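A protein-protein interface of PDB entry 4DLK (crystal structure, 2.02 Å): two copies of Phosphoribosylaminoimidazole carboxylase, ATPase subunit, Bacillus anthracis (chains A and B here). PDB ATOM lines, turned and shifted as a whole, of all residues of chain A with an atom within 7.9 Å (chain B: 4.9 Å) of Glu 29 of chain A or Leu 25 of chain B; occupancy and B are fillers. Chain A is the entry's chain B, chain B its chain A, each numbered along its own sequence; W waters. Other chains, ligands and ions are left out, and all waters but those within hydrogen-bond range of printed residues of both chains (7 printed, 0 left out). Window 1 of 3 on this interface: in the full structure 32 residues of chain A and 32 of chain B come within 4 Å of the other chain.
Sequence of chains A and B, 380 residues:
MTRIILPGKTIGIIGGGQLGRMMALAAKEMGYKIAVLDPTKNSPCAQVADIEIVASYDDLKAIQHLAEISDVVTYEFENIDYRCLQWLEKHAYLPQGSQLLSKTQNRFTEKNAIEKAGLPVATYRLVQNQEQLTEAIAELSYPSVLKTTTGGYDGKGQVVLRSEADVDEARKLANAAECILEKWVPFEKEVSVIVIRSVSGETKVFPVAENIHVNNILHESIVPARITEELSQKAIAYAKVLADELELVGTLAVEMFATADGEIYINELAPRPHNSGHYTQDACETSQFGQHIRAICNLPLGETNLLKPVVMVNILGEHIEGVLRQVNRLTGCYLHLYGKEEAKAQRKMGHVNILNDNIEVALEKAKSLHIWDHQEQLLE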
ATOM      1  N   PRO A   7      -3.892   3.348 -21.257  1.00  0.00           N
ATOM      2  CA  PRO A   7      -3.144   2.961 -20.062  1.00  0.00           C
ATOM      3  C   PRO A   7      -3.867   1.859 -19.298  1.00  0.00           C
ATOM      4  O   PRO A   7      -5.096   1.862 -19.227  1.00  0.00           O
ATOM      5  CB  PRO A   7      -3.113   4.251 -19.250  1.00  0.00           C
ATOM      6  CG  PRO A   7      -3.093   5.323 -20.286  1.00  0.00           C
ATOM      7  CD  PRO A   7      -4.001   4.818 -21.379  1.00  0.00           C
ATOM      8  N   ARG A  21      14.219  -1.259 -21.935  1.00  0.00           N
ATOM      9  CA  ARG A  21      14.139  -0.923 -20.511  1.00  0.00           C
ATOM     10  C   ARG A  21      13.622   0.503 -20.328  1.00  0.00           C
ATOM     11  O   ARG A  21      12.755   0.761 -19.492  1.00  0.00           O
ATOM     12  CB  ARG A  21      15.508  -1.096 -19.825  1.00  0.00           C
ATOM     13  CG  ARG A  21      15.577  -0.594 -18.377  1.00  0.00           C
ATOM     14  CD  ARG A  21      17.021  -0.574 -17.891  1.00  0.00           C
ATOM     15  NE  ARG A  21      17.198  -0.174 -16.490  1.00  0.00           N
ATOM     16  CZ  ARG A  21      17.200  -1.017 -15.456  1.00  0.00           C
ATOM     17  NH1 ARG A  21      16.994  -2.318 -15.646  1.00  0.00           N
ATOM     18  NH2 ARG A  21      17.399  -0.559 -14.223  1.00  0.00           N
ATOM     19  N   MET A  23      11.952   2.327 -22.593  1.00  0.00           N
ATOM     20  CA  MET A  23      10.546   2.309 -23.041  1.00  0.00           C
ATOM     21  C   MET A  23       9.624   1.856 -21.911  1.00  0.00           C
ATOM     22  O   MET A  23       8.574   2.456 -21.663  1.00  0.00           O
ATOM     23  CB  MET A  23      10.348   1.340 -24.212  1.00  0.00           C
ATOM     24  CG  MET A  23      10.912   1.777 -25.552  1.00  0.00           C
ATOM     25  SD  MET A  23      10.548   0.446 -26.721  1.00  0.00           S
ATOM     26  CE  MET A  23      11.452   1.015 -28.161  1.00  0.00           C
ATOM     27  N   ALA A  24      10.020   0.777 -21.245  1.00  0.00           N
ATOM     28  CA  ALA A  24       9.219   0.178 -20.177  1.00  0.00           C
ATOM     29  C   ALA A  24       9.032   1.104 -18.973  1.00  0.00           C
ATOM     30  O   ALA A  24       7.929   1.200 -18.423  1.00  0.00           O
ATOM     31  CB  ALA A  24       9.822  -1.148 -19.748  1.00  0.00           C
ATOM     32  N   LEU A  25      10.105   1.791 -18.570  1.00  0.00           N
ATOM     33  CA  LEU A  25      10.033   2.748 -17.463  1.00  0.00           C
ATOM     34  C   LEU A  25       9.059   3.895 -17.751  1.00  0.00           C
ATOM     35  O   LEU A  25       8.235   4.238 -16.899  1.00  0.00           O
ATOM     36  CB  LEU A  25      11.428   3.279 -17.109  1.00  0.00           C
ATOM     37  CG  LEU A  25      12.341   2.227 -16.461  1.00  0.00           C
ATOM     38  CD1 LEU A  25      13.810   2.607 -16.572  1.00  0.00           C
ATOM     39  CD2 LEU A  25      11.948   1.968 -15.010  1.00  0.00           C
ATOM     40  N   ALA A  26       9.157   4.466 -18.955  1.00  0.00           N
ATOM     41  CA  ALA A  26       8.239   5.505 -19.414  1.00  0.00           C
ATOM     42  C   ALA A  26       6.809   4.980 -19.541  1.00  0.00           C
ATOM     43  O   ALA A  26       5.860   5.690 -19.221  1.00  0.00           O
ATOM     44  CB  ALA A  26       8.717   6.107 -20.733  1.00  0.00           C
ATOM     45  N   ALA A  27       6.654   3.733 -19.987  1.00  0.00           N
ATOM     46  CA  ALA A  27       5.324   3.123 -20.076  1.00  0.00           C
ATOM     47  C   ALA A  27       4.700   2.920 -18.693  1.00  0.00           C
ATOM     48  O   ALA A  27       3.502   3.146 -18.506  1.00  0.00           O
ATOM     49  CB  ALA A  27       5.376   1.807 -20.842  1.00  0.00           C
ATOM     50  N   LYS A  28       5.523   2.508 -17.731  1.00  0.00           N
ATOM     51  CA  LYS A  28       5.059   2.245 -16.370  1.00  0.00           C
ATOM     52  C   LYS A  28       4.559   3.488 -15.639  1.00  0.00           C
ATOM     53  O   LYS A  28       3.613   3.396 -14.859  1.00  0.00           O
ATOM     54  CB  LYS A  28       6.126   1.511 -15.552  1.00  0.00           C
ATOM     55  CG  LYS A  28       6.260   0.053 -15.956  1.00  0.00           C
ATOM     56  CD  LYS A  28       6.275  -0.854 -14.742  1.00  0.00           C
ATOM     57  CE  LYS A  28       5.827  -2.253 -15.130  1.00  0.00           C
ATOM     58  NZ  LYS A  28       5.077  -2.902 -14.022  1.00  0.00           N
ATOM     59  N   GLU A  29       5.178   4.641 -15.903  1.00  0.00           N
ATOM     60  CA  GLU A  29       4.728   5.914 -15.331  1.00  0.00           C
ATOM     61  C   GLU A  29       3.300   6.247 -15.743  1.00  0.00           C
ATOM     62  O   GLU A  29       2.543   6.825 -14.963  1.00  0.00           O
ATOM     63  CB  GLU A  29       5.650   7.070 -15.732  1.00  0.00           C
ATOM     64  CG  GLU A  29       7.001   7.084 -15.034  1.00  0.00           C
ATOM     65  CD  GLU A  29       6.961   7.627 -13.608  1.00  0.00           C
ATOM     66  OE1 GLU A  29       5.866   7.979 -13.100  1.00  0.00           O
ATOM     67  OE2 GLU A  29       8.044   7.700 -12.983  1.00  0.00           O
ATOM     68  N   MET A  30       2.947   5.875 -16.972  1.00  0.00           N
ATOM     69  CA  MET A  30       1.601   6.069 -17.497  1.00  0.00           C
ATOM     70  C   MET A  30       0.631   4.947 -17.122  1.00  0.00           C
ATOM     71  O   MET A  30      -0.550   5.011 -17.470  1.00  0.00           O
ATOM     72  CB  MET A  30       1.645   6.247 -19.014  1.00  0.00           C
ATOM     73  CG  MET A  30       2.163   7.605 -19.451  1.00  0.00           C
ATOM     74  SD  MET A  30       2.076   7.872 -21.238  1.00  0.00           S
ATOM     75  CE  MET A  30       3.515   6.947 -21.776  1.00  0.00           C
ATOM     76  N   GLY A  31       1.125   3.925 -16.425  1.00  0.00           N
ATOM     77  CA  GLY A  31       0.280   2.828 -15.935  1.00  0.00           C
ATOM     78  C   GLY A  31       0.091   1.666 -16.897  1.00  0.00           C
ATOM     79  O   GLY A  31      -0.856   0.886 -16.763  1.00  0.00           O
ATOM     80  N   TYR A  32       0.993   1.545 -17.867  1.00  0.00           N
ATOM     81  CA  TYR A  32       1.009   0.391 -18.757  1.00  0.00           C
ATOM     82  C   TYR A  32       1.704  -0.791 -18.101  1.00  0.00           C
ATOM     83  O   TYR A  32       2.602  -0.610 -17.277  1.00  0.00           O
ATOM     84  CB  TYR A  32       1.720   0.736 -20.067  1.00  0.00           C
ATOM     85  CG  TYR A  32       0.924   1.641 -20.975  1.00  0.00           C
ATOM     86  CD1 TYR A  32      -0.095   1.131 -21.793  1.00  0.00           C
ATOM     87  CD2 TYR A  32       1.185   3.009 -21.024  1.00  0.00           C
ATOM     88  CE1 TYR A  32      -0.823   1.966 -22.635  1.00  0.00           C
ATOM     89  CE2 TYR A  32       0.462   3.852 -21.854  1.00  0.00           C
ATOM     90  CZ  TYR A  32      -0.542   3.329 -22.661  1.00  0.00           C
ATOM     91  OH  TYR A  32      -1.254   4.183 -23.486  1.00  0.00           O
ATOM     92  N   VAL A  48      12.496  -4.576 -15.390  1.00  0.00           N
ATOM     93  CA  VAL A  48      11.400  -3.624 -15.200  1.00  0.00           C
ATOM     94  C   VAL A  48      10.039  -4.183 -15.625  1.00  0.00           C
ATOM     95  O   VAL A  48       9.004  -3.715 -15.153  1.00  0.00           O
ATOM     96  CB  VAL A  48      11.681  -2.256 -15.873  1.00  0.00           C
ATOM     97  CG1 VAL A  48      12.896  -1.597 -15.242  1.00  0.00           C
ATOM     98  CG2 VAL A  48      11.905  -2.408 -17.365  1.00  0.00           C
ATOM     99  N   ARG A 294       3.705   6.857 -26.644  1.00  0.00           N
ATOM    100  CA  ARG A 294       2.550   7.654 -27.058  1.00  0.00           C
ATOM    101  C   ARG A 294       2.241   7.465 -28.544  1.00  0.00           C
ATOM    102  O   ARG A 294       1.075   7.394 -28.934  1.00  0.00           O
ATOM    103  CB  ARG A 294       2.769   9.141 -26.748  1.00  0.00           C
ATOM    104  CG  ARG A 294       2.599   9.504 -25.277  1.00  0.00           C
ATOM    105  CD  ARG A 294       3.151  10.893 -24.977  1.00  0.00           C
ATOM    106  NE  ARG A 294       2.816  11.295 -23.614  1.00  0.00           N
ATOM    107  CZ  ARG A 294       3.532  10.975 -22.535  1.00  0.00           C
ATOM    108  NH1 ARG A 294       4.651  10.264 -22.652  1.00  0.00           N
ATOM    109  NH2 ARG A 294       3.128  11.369 -21.333  1.00  0.00           N
ATOM    110  N   ARG B  21       6.187   3.362  -5.473  1.00  0.00           N
ATOM    111  CA  ARG B  21       6.327   3.066  -6.894  1.00  0.00           C
ATOM    112  C   ARG B  21       7.189   4.103  -7.615  1.00  0.00           C
ATOM    113  O   ARG B  21       8.085   3.749  -8.383  1.00  0.00           O
ATOM    114  CB  ARG B  21       4.954   2.968  -7.568  1.00  0.00           C
ATOM    115  CG  ARG B  21       4.994   2.772  -9.083  1.00  0.00           C
ATOM    116  CD  ARG B  21       3.574   2.901  -9.614  1.00  0.00           C
ATOM    117  NE  ARG B  21       3.432   2.744 -11.061  1.00  0.00           N
ATOM    118  CZ  ARG B  21       3.189   1.587 -11.679  1.00  0.00           C
ATOM    119  NH1 ARG B  21       3.122   0.449 -10.994  1.00  0.00           N
ATOM    120  NH2 ARG B  21       3.044   1.560 -12.998  1.00  0.00           N
ATOM    121  N   MET B  22       6.908   5.376  -7.371  1.00  0.00           N
ATOM    122  CA  MET B  22       7.640   6.459  -8.027  1.00  0.00           C
ATOM    123  C   MET B  22       9.092   6.606  -7.551  1.00  0.00           C
ATOM    124  O   MET B  22       9.973   6.955  -8.346  1.00  0.00           O
ATOM    125  CB  MET B  22       6.849   7.762  -7.935  1.00  0.00           C
ATOM    126  CG  MET B  22       5.584   7.716  -8.788  1.00  0.00           C
ATOM    127  SD  MET B  22       4.619   9.236  -8.825  1.00  0.00           S
ATOM    128  CE  MET B  22       3.667   9.131  -7.315  1.00  0.00           C
ATOM    129  N   MET B  23       9.338   6.333  -6.267  1.00  0.00           N
ATOM    130  CA  MET B  23      10.699   6.125  -5.765  1.00  0.00           C
ATOM    131  C   MET B  23      11.406   5.025  -6.561  1.00  0.00           C
ATOM    132  O   MET B  23      12.543   5.203  -7.007  1.00  0.00           O
ATOM    133  CB  MET B  23      10.684   5.685  -4.300  1.00  0.00           C
ATOM    134  CG  MET B  23      10.423   6.773  -3.277  1.00  0.00           C
ATOM    135  SD  MET B  23      10.434   6.027  -1.625  1.00  0.00           S
ATOM    136  CE  MET B  23       9.926   7.448  -0.667  1.00  0.00           C
ATOM    137  N   ALA B  24      10.731   3.880  -6.699  1.00  0.00           N
ATOM    138  CA  ALA B  24      11.318   2.708  -7.354  1.00  0.00           C
ATOM    139  C   ALA B  24      11.641   3.003  -8.815  1.00  0.00           C
ATOM    140  O   ALA B  24      12.678   2.594  -9.312  1.00  0.00           O
ATOM    141  CB  ALA B  24      10.387   1.502  -7.246  1.00  0.00           C
ATOM    142  N   LEU B  25      10.747   3.714  -9.499  1.00  0.00           N
ATOM    143  CA  LEU B  25      10.969   4.047 -10.909  1.00  0.00           C
ATOM    144  C   LEU B  25      12.194   4.934 -11.080  1.00  0.00           C
ATOM    145  O   LEU B  25      13.039   4.673 -11.935  1.00  0.00           O
ATOM    146  CB  LEU B  25       9.723   4.680 -11.540  1.00  0.00           C
ATOM    147  CG  LEU B  25       8.575   3.687 -11.749  1.00  0.00           C
ATOM    148  CD1 LEU B  25       7.277   4.408 -12.086  1.00  0.00           C
ATOM    149  CD2 LEU B  25       8.924   2.665 -12.826  1.00  0.00           C
ATOM    150  N   ALA B  26      12.303   5.958 -10.241  1.00  0.00           N
ATOM    151  CA  ALA B  26      13.459   6.863 -10.283  1.00  0.00           C
ATOM    152  C   ALA B  26      14.760   6.119  -9.953  1.00  0.00           C
ATOM    153  O   ALA B  26      15.803   6.343 -10.591  1.00  0.00           O
ATOM    154  CB  ALA B  26      13.240   8.044  -9.347  1.00  0.00           C
ATOM    155  N   ALA B  27      14.696   5.199  -8.989  1.00  0.00           N
ATOM    156  CA  ALA B  27      15.862   4.410  -8.624  1.00  0.00           C
ATOM    157  C   ALA B  27      16.298   3.451  -9.736  1.00  0.00           C
ATOM    158  O   ALA B  27      17.496   3.251  -9.954  1.00  0.00           O
ATOM    159  CB  ALA B  27      15.615   3.653  -7.320  1.00  0.00           C
ATOM    160  N   LYS B  28      15.323   2.873 -10.442  1.00  0.00           N
ATOM    161  CA  LYS B  28      15.608   1.981 -11.572  1.00  0.00           C
ATOM    162  C   LYS B  28      16.384   2.674 -12.701  1.00  0.00           C
ATOM    163  O   LYS B  28      17.316   2.094 -13.273  1.00  0.00           O
ATOM    164  CB  LYS B  28      14.311   1.364 -12.110  1.00  0.00           C
ATOM    165  CG  LYS B  28      13.782   0.219 -11.258  1.00  0.00           C
ATOM    166  CD  LYS B  28      14.424  -1.096 -11.658  1.00  0.00           C
ATOM    167  CE  LYS B  28      13.815  -2.244 -10.868  1.00  0.00           C
ATOM    168  NZ  LYS B  28      14.511  -3.515 -11.189  1.00  0.00           N
ATOM    169  N   GLU B  29      16.003   3.908 -13.017  1.00  0.00           N
ATOM    170  CA  GLU B  29      16.748   4.696 -14.006  1.00  0.00           C
ATOM    171  C   GLU B  29      18.242   4.727 -13.674  1.00  0.00           C
ATOM    172  O   GLU B  29      19.081   4.664 -14.574  1.00  0.00           O
ATOM    173  CB  GLU B  29      16.193   6.120 -14.135  1.00  0.00           C
ATOM    174  CG  GLU B  29      14.883   6.229 -14.920  1.00  0.00           C
ATOM    175  CD  GLU B  29      15.028   6.042 -16.435  1.00  0.00           C
ATOM    176  OE1 GLU B  29      16.165   5.949 -16.971  1.00  0.00           O
ATOM    177  OE2 GLU B  29      13.977   5.997 -17.118  1.00  0.00           O
ATOM    178  N   VAL B  48       6.909  -2.758  -9.805  1.00  0.00           N
ATOM    179  CA  VAL B  48       8.154  -2.184 -10.307  1.00  0.00           C
ATOM    180  C   VAL B  48       9.351  -2.822  -9.578  1.00  0.00           C
ATOM    181  O   VAL B  48      10.480  -2.763 -10.054  1.00  0.00           O
ATOM    182  CB  VAL B  48       8.148  -0.636 -10.129  1.00  0.00           C
ATOM    183  CG1 VAL B  48       9.475  -0.022 -10.542  1.00  0.00           C
ATOM    184  CG2 VAL B  48       7.010  -0.003 -10.926  1.00  0.00           C
ATOM    185  N   GLN B 281       8.080  15.836 -11.257  1.00  0.00           N
ATOM    186  CA  GLN B 281       8.358  14.766 -12.226  1.00  0.00           C
ATOM    187  C   GLN B 281       8.519  15.279 -13.658  1.00  0.00           C
ATOM    188  O   GLN B 281       9.313  14.738 -14.429  1.00  0.00           O
ATOM    189  CB  GLN B 281       7.239  13.737 -12.210  1.00  0.00           C
ATOM    190  CG  GLN B 281       7.211  12.833 -10.998  1.00  0.00           C
ATOM    191  CD  GLN B 281       6.241  11.700 -11.214  1.00  0.00           C
ATOM    192  OE1 GLN B 281       5.039  11.924 -11.380  1.00  0.00           O
ATOM    193  NE2 GLN B 281       6.754  10.480 -11.255  1.00  0.00           N
ATOM    194  N   LEU B 335       0.522  12.456 -18.186  1.00  0.00           N
ATOM    195  CA  LEU B 335      -0.273  11.527 -17.385  1.00  0.00           C
ATOM    196  C   LEU B 335       0.583  10.542 -16.585  1.00  0.00           C
ATOM    197  O   LEU B 335       1.545   9.976 -17.104  1.00  0.00           O
ATOM    198  CB  LEU B 335      -1.234  10.758 -18.308  1.00  0.00           C
ATOM    199  CG  LEU B 335      -2.105   9.623 -17.760  1.00  0.00           C
ATOM    200  CD1 LEU B 335      -3.139  10.140 -16.774  1.00  0.00           C
ATOM    201  CD2 LEU B 335      -2.786   8.884 -18.903  1.00  0.00           C
ATOM    202  N   HIS B 336       0.213  10.343 -15.322  1.00  0.00           N
ATOM    203  CA  HIS B 336       0.849   9.360 -14.459  1.00  0.00           C
ATOM    204  C   HIS B 336      -0.210   8.524 -13.826  1.00  0.00           C
ATOM    205  O   HIS B 336      -1.129   9.056 -13.208  1.00  0.00           O
ATOM    206  CB  HIS B 336       1.686  10.050 -13.391  1.00  0.00           C
ATOM    207  CG  HIS B 336       2.867  10.806 -13.945  1.00  0.00           C
ATOM    208  ND1 HIS B 336       4.100  10.274 -14.005  1.00  0.00           N
ATOM    209  CD2 HIS B 336       2.960  12.085 -14.494  1.00  0.00           C
ATOM    210  CE1 HIS B 336       4.947  11.170 -14.551  1.00  0.00           C
ATOM    211  NE2 HIS B 336       4.247  12.278 -14.850  1.00  0.00           N
ATOM    212  N   LEU B 337      -0.122   7.210 -14.005  1.00  0.00           N
ATOM    213  CA  LEU B 337      -1.084   6.291 -13.406  1.00  0.00           C
ATOM    214  C   LEU B 337      -0.356   5.216 -12.618  1.00  0.00           C
ATOM    215  O   LEU B 337       0.648   4.661 -13.073  1.00  0.00           O
ATOM    216  CB  LEU B 337      -2.033   5.683 -14.458  1.00  0.00           C
ATOM    217  CG  LEU B 337      -3.045   6.641 -15.118  1.00  0.00           C
ATOM    218  CD1 LEU B 337      -3.767   5.951 -16.265  1.00  0.00           C
ATOM    219  CD2 LEU B 337      -4.057   7.216 -14.129  1.00  0.00           C
HETATM  220  O   HOH W   1      17.511  -2.284 -11.807  1.00  0.00           O
HETATM  221  O   HOH W   2      17.998   2.411 -16.559  1.00  0.00           O
HETATM  222  O   HOH W   3       9.485   8.520 -10.561  1.00  0.00           O
HETATM  223  O   HOH W   4       0.275  12.126 -21.269  1.00  0.00           O
HETATM  224  O   HOH W   5       4.062  10.470 -18.572  1.00  0.00           O
HETATM  225  O   HOH W   6       3.722   7.920 -11.780  1.00  0.00           O
HETATM  226  O   HOH W   7       2.473  -0.805 -14.497  1.00  0.00           O
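The backbone carbonyl oxygen (O) of Leu 337 of chain B lies close to the backbone NH (N) of Gly 31 of chain A (3.5 Å). The backbone carbonyl oxygen (O) of Lys 28 of chain B sits at hydrogen-bond distance from the guanidinium group (NH2) of Arg 21 of chain A (2.8 Å). The side-chain amide nitrogen (NE2) of Gln 281 of chain B is in hydrogen-bond range of the side-chain carboxylate (OE1) of Glu 29 of chain A, 3.2 Å away. N of Leu 337 of chain B lies within hydrogen-bond range of O of Glu 29 of chain A, 2.9 Å away. The guanidinium group (NH2) of Arg 21 of chain B sits at hydrogen-bond distance from the backbone carbonyl oxygen (O) of Lys 28 of chain A (2.7 Å). OE1 of Glu 29 of chain A lies within hydrogen-bond range of ND1 of His 336 of chain B.
NE2 of Gln 281 of chain B is in hydrogen-bond range of SD of Met 22 of chain B. The side-chain sulfur (SD) of Met 30 of chain A is in hydrogen-bond range of the guanidinium group (NH2) of Arg 294 of chain A, 3.7 Å away. OE1 of Gln 281 of chain B is in hydrogen-bond range of ND1 of His 336 of chain B, at 3.2 Å.
Pro 7 of chain A touches Leu 335 of chain B (CG to CD2, 3.8 Å). Leu 337 of chain B touches Pro 7 of chain A. Leu 25 of chain A touches Lys 28 of chain B (CD2 to CB, 3.8 Å). OE2 of Glu 29 of chain B touches CD1 of Leu 25 of chain A, 3.4 Å away. Lys 28 of chain A touches Val 48 of chain B. O of Lys 28 of chain A touches O of Leu 337 of chain B, at 3.7 Å. Glu 29 of chain A touches Leu 25 of chain B. O of Leu 335 of chain B touches O of Glu 29 of chain A, 3.9 Å away. Met 30 of chain A touches Leu 335 of chain B (CG to O, 3.4 Å). Met 30 of chain A touches Leu 337 of chain B.
Of the printed residues of chain B, Pro 7 of chain A touches Leu 335 and Leu 337. Printed residues of chain B within 4 Å of Lys 28 of chain A: Arg 21, Val 48 and Leu 337. Glu 29 of chain A touches just these residues of chain B: Leu 25, Gln 281, Leu 335, His 336 and Leu 337. Printed residues of chain B within 4 Å of Val 48 of chain A: Lys 28 (3.9 Å). No residue of chain A comes within 4 Å of Ala 24 of chain B. Leu 25 of chain B touches just these residues of chain A: Leu 25 and Glu 29. No residue of chain A comes within 4 Å of Ala 26 of chain B. Ala 27 of chain B touches none of the printed residues of chain A. Of the printed residues of chain A, Gln 281 of chain B touches Glu 29.
Of the 14 printed residues of chain B, 9 touch a printed residue of chain A. Hydrophobic or aromatic side chains of chain B that line the printed part of chain A: Leu 25, Val 48, Leu 335, His 336 and Leu 337. Hydrophobic or aromatic side chains of chain A within 4 Å of the printed part of chain B: Pro 7, Leu 25, Met 30 and Val 48.
Arg 21 of chain A touches Lys 28 of chain B, and with the chains exchanged Lys 28 of chain A touches Arg 21 of chain B. Leu 25 of chain A touches its own counterpart, Leu 25 of chain B. Leu 25 of chain A touches Glu 29 of chain B, and with the chains exchanged Glu 29 of chain A touches Leu 25 of chain B. Lys 28 of chain A touches Val 48 of chain B, and with the chains exchanged Val 48 of chain A touches Lys 28 of chain B.
Water W6 lies within hydrogen-bond range of OE1 of Glu 29 of chain A (2.5 Å), ND1 of His 336 of chain B (3.3 Å) and SD of Met 22 of chain B (3.4 Å). Water W2 lies within hydrogen-bond range of NE of Arg 21 of chain A (2.7 Å), O of Glu 29 of chain B (3.2 Å) and O of Lys 28 of chain B (3.4 Å). Water W3 lies within hydrogen-bond range of the backbone carbonyl oxygen of Met 22 of chain B, the side-chain carboxylate of Glu 29 of chain A and the side-chain amide nitrogen of Gln 281 of chain B. Water W7 lies within hydrogen-bond range of O of Tyr 32 of chain A (2.8 Å), NH2 of Arg 21 of chain B (2.9 Å) and NZ of Lys 28 of chain A (3.4 Å). Water W5 bridges the backbone carbonyl oxygen of Leu 335 of chain B (3.0 Å) and the guanidinium group of Arg 294 of chain A (3.1 Å). Water W1 bridges NH2 of Arg 21 of chain A and NZ of Lys 28 of chain B.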
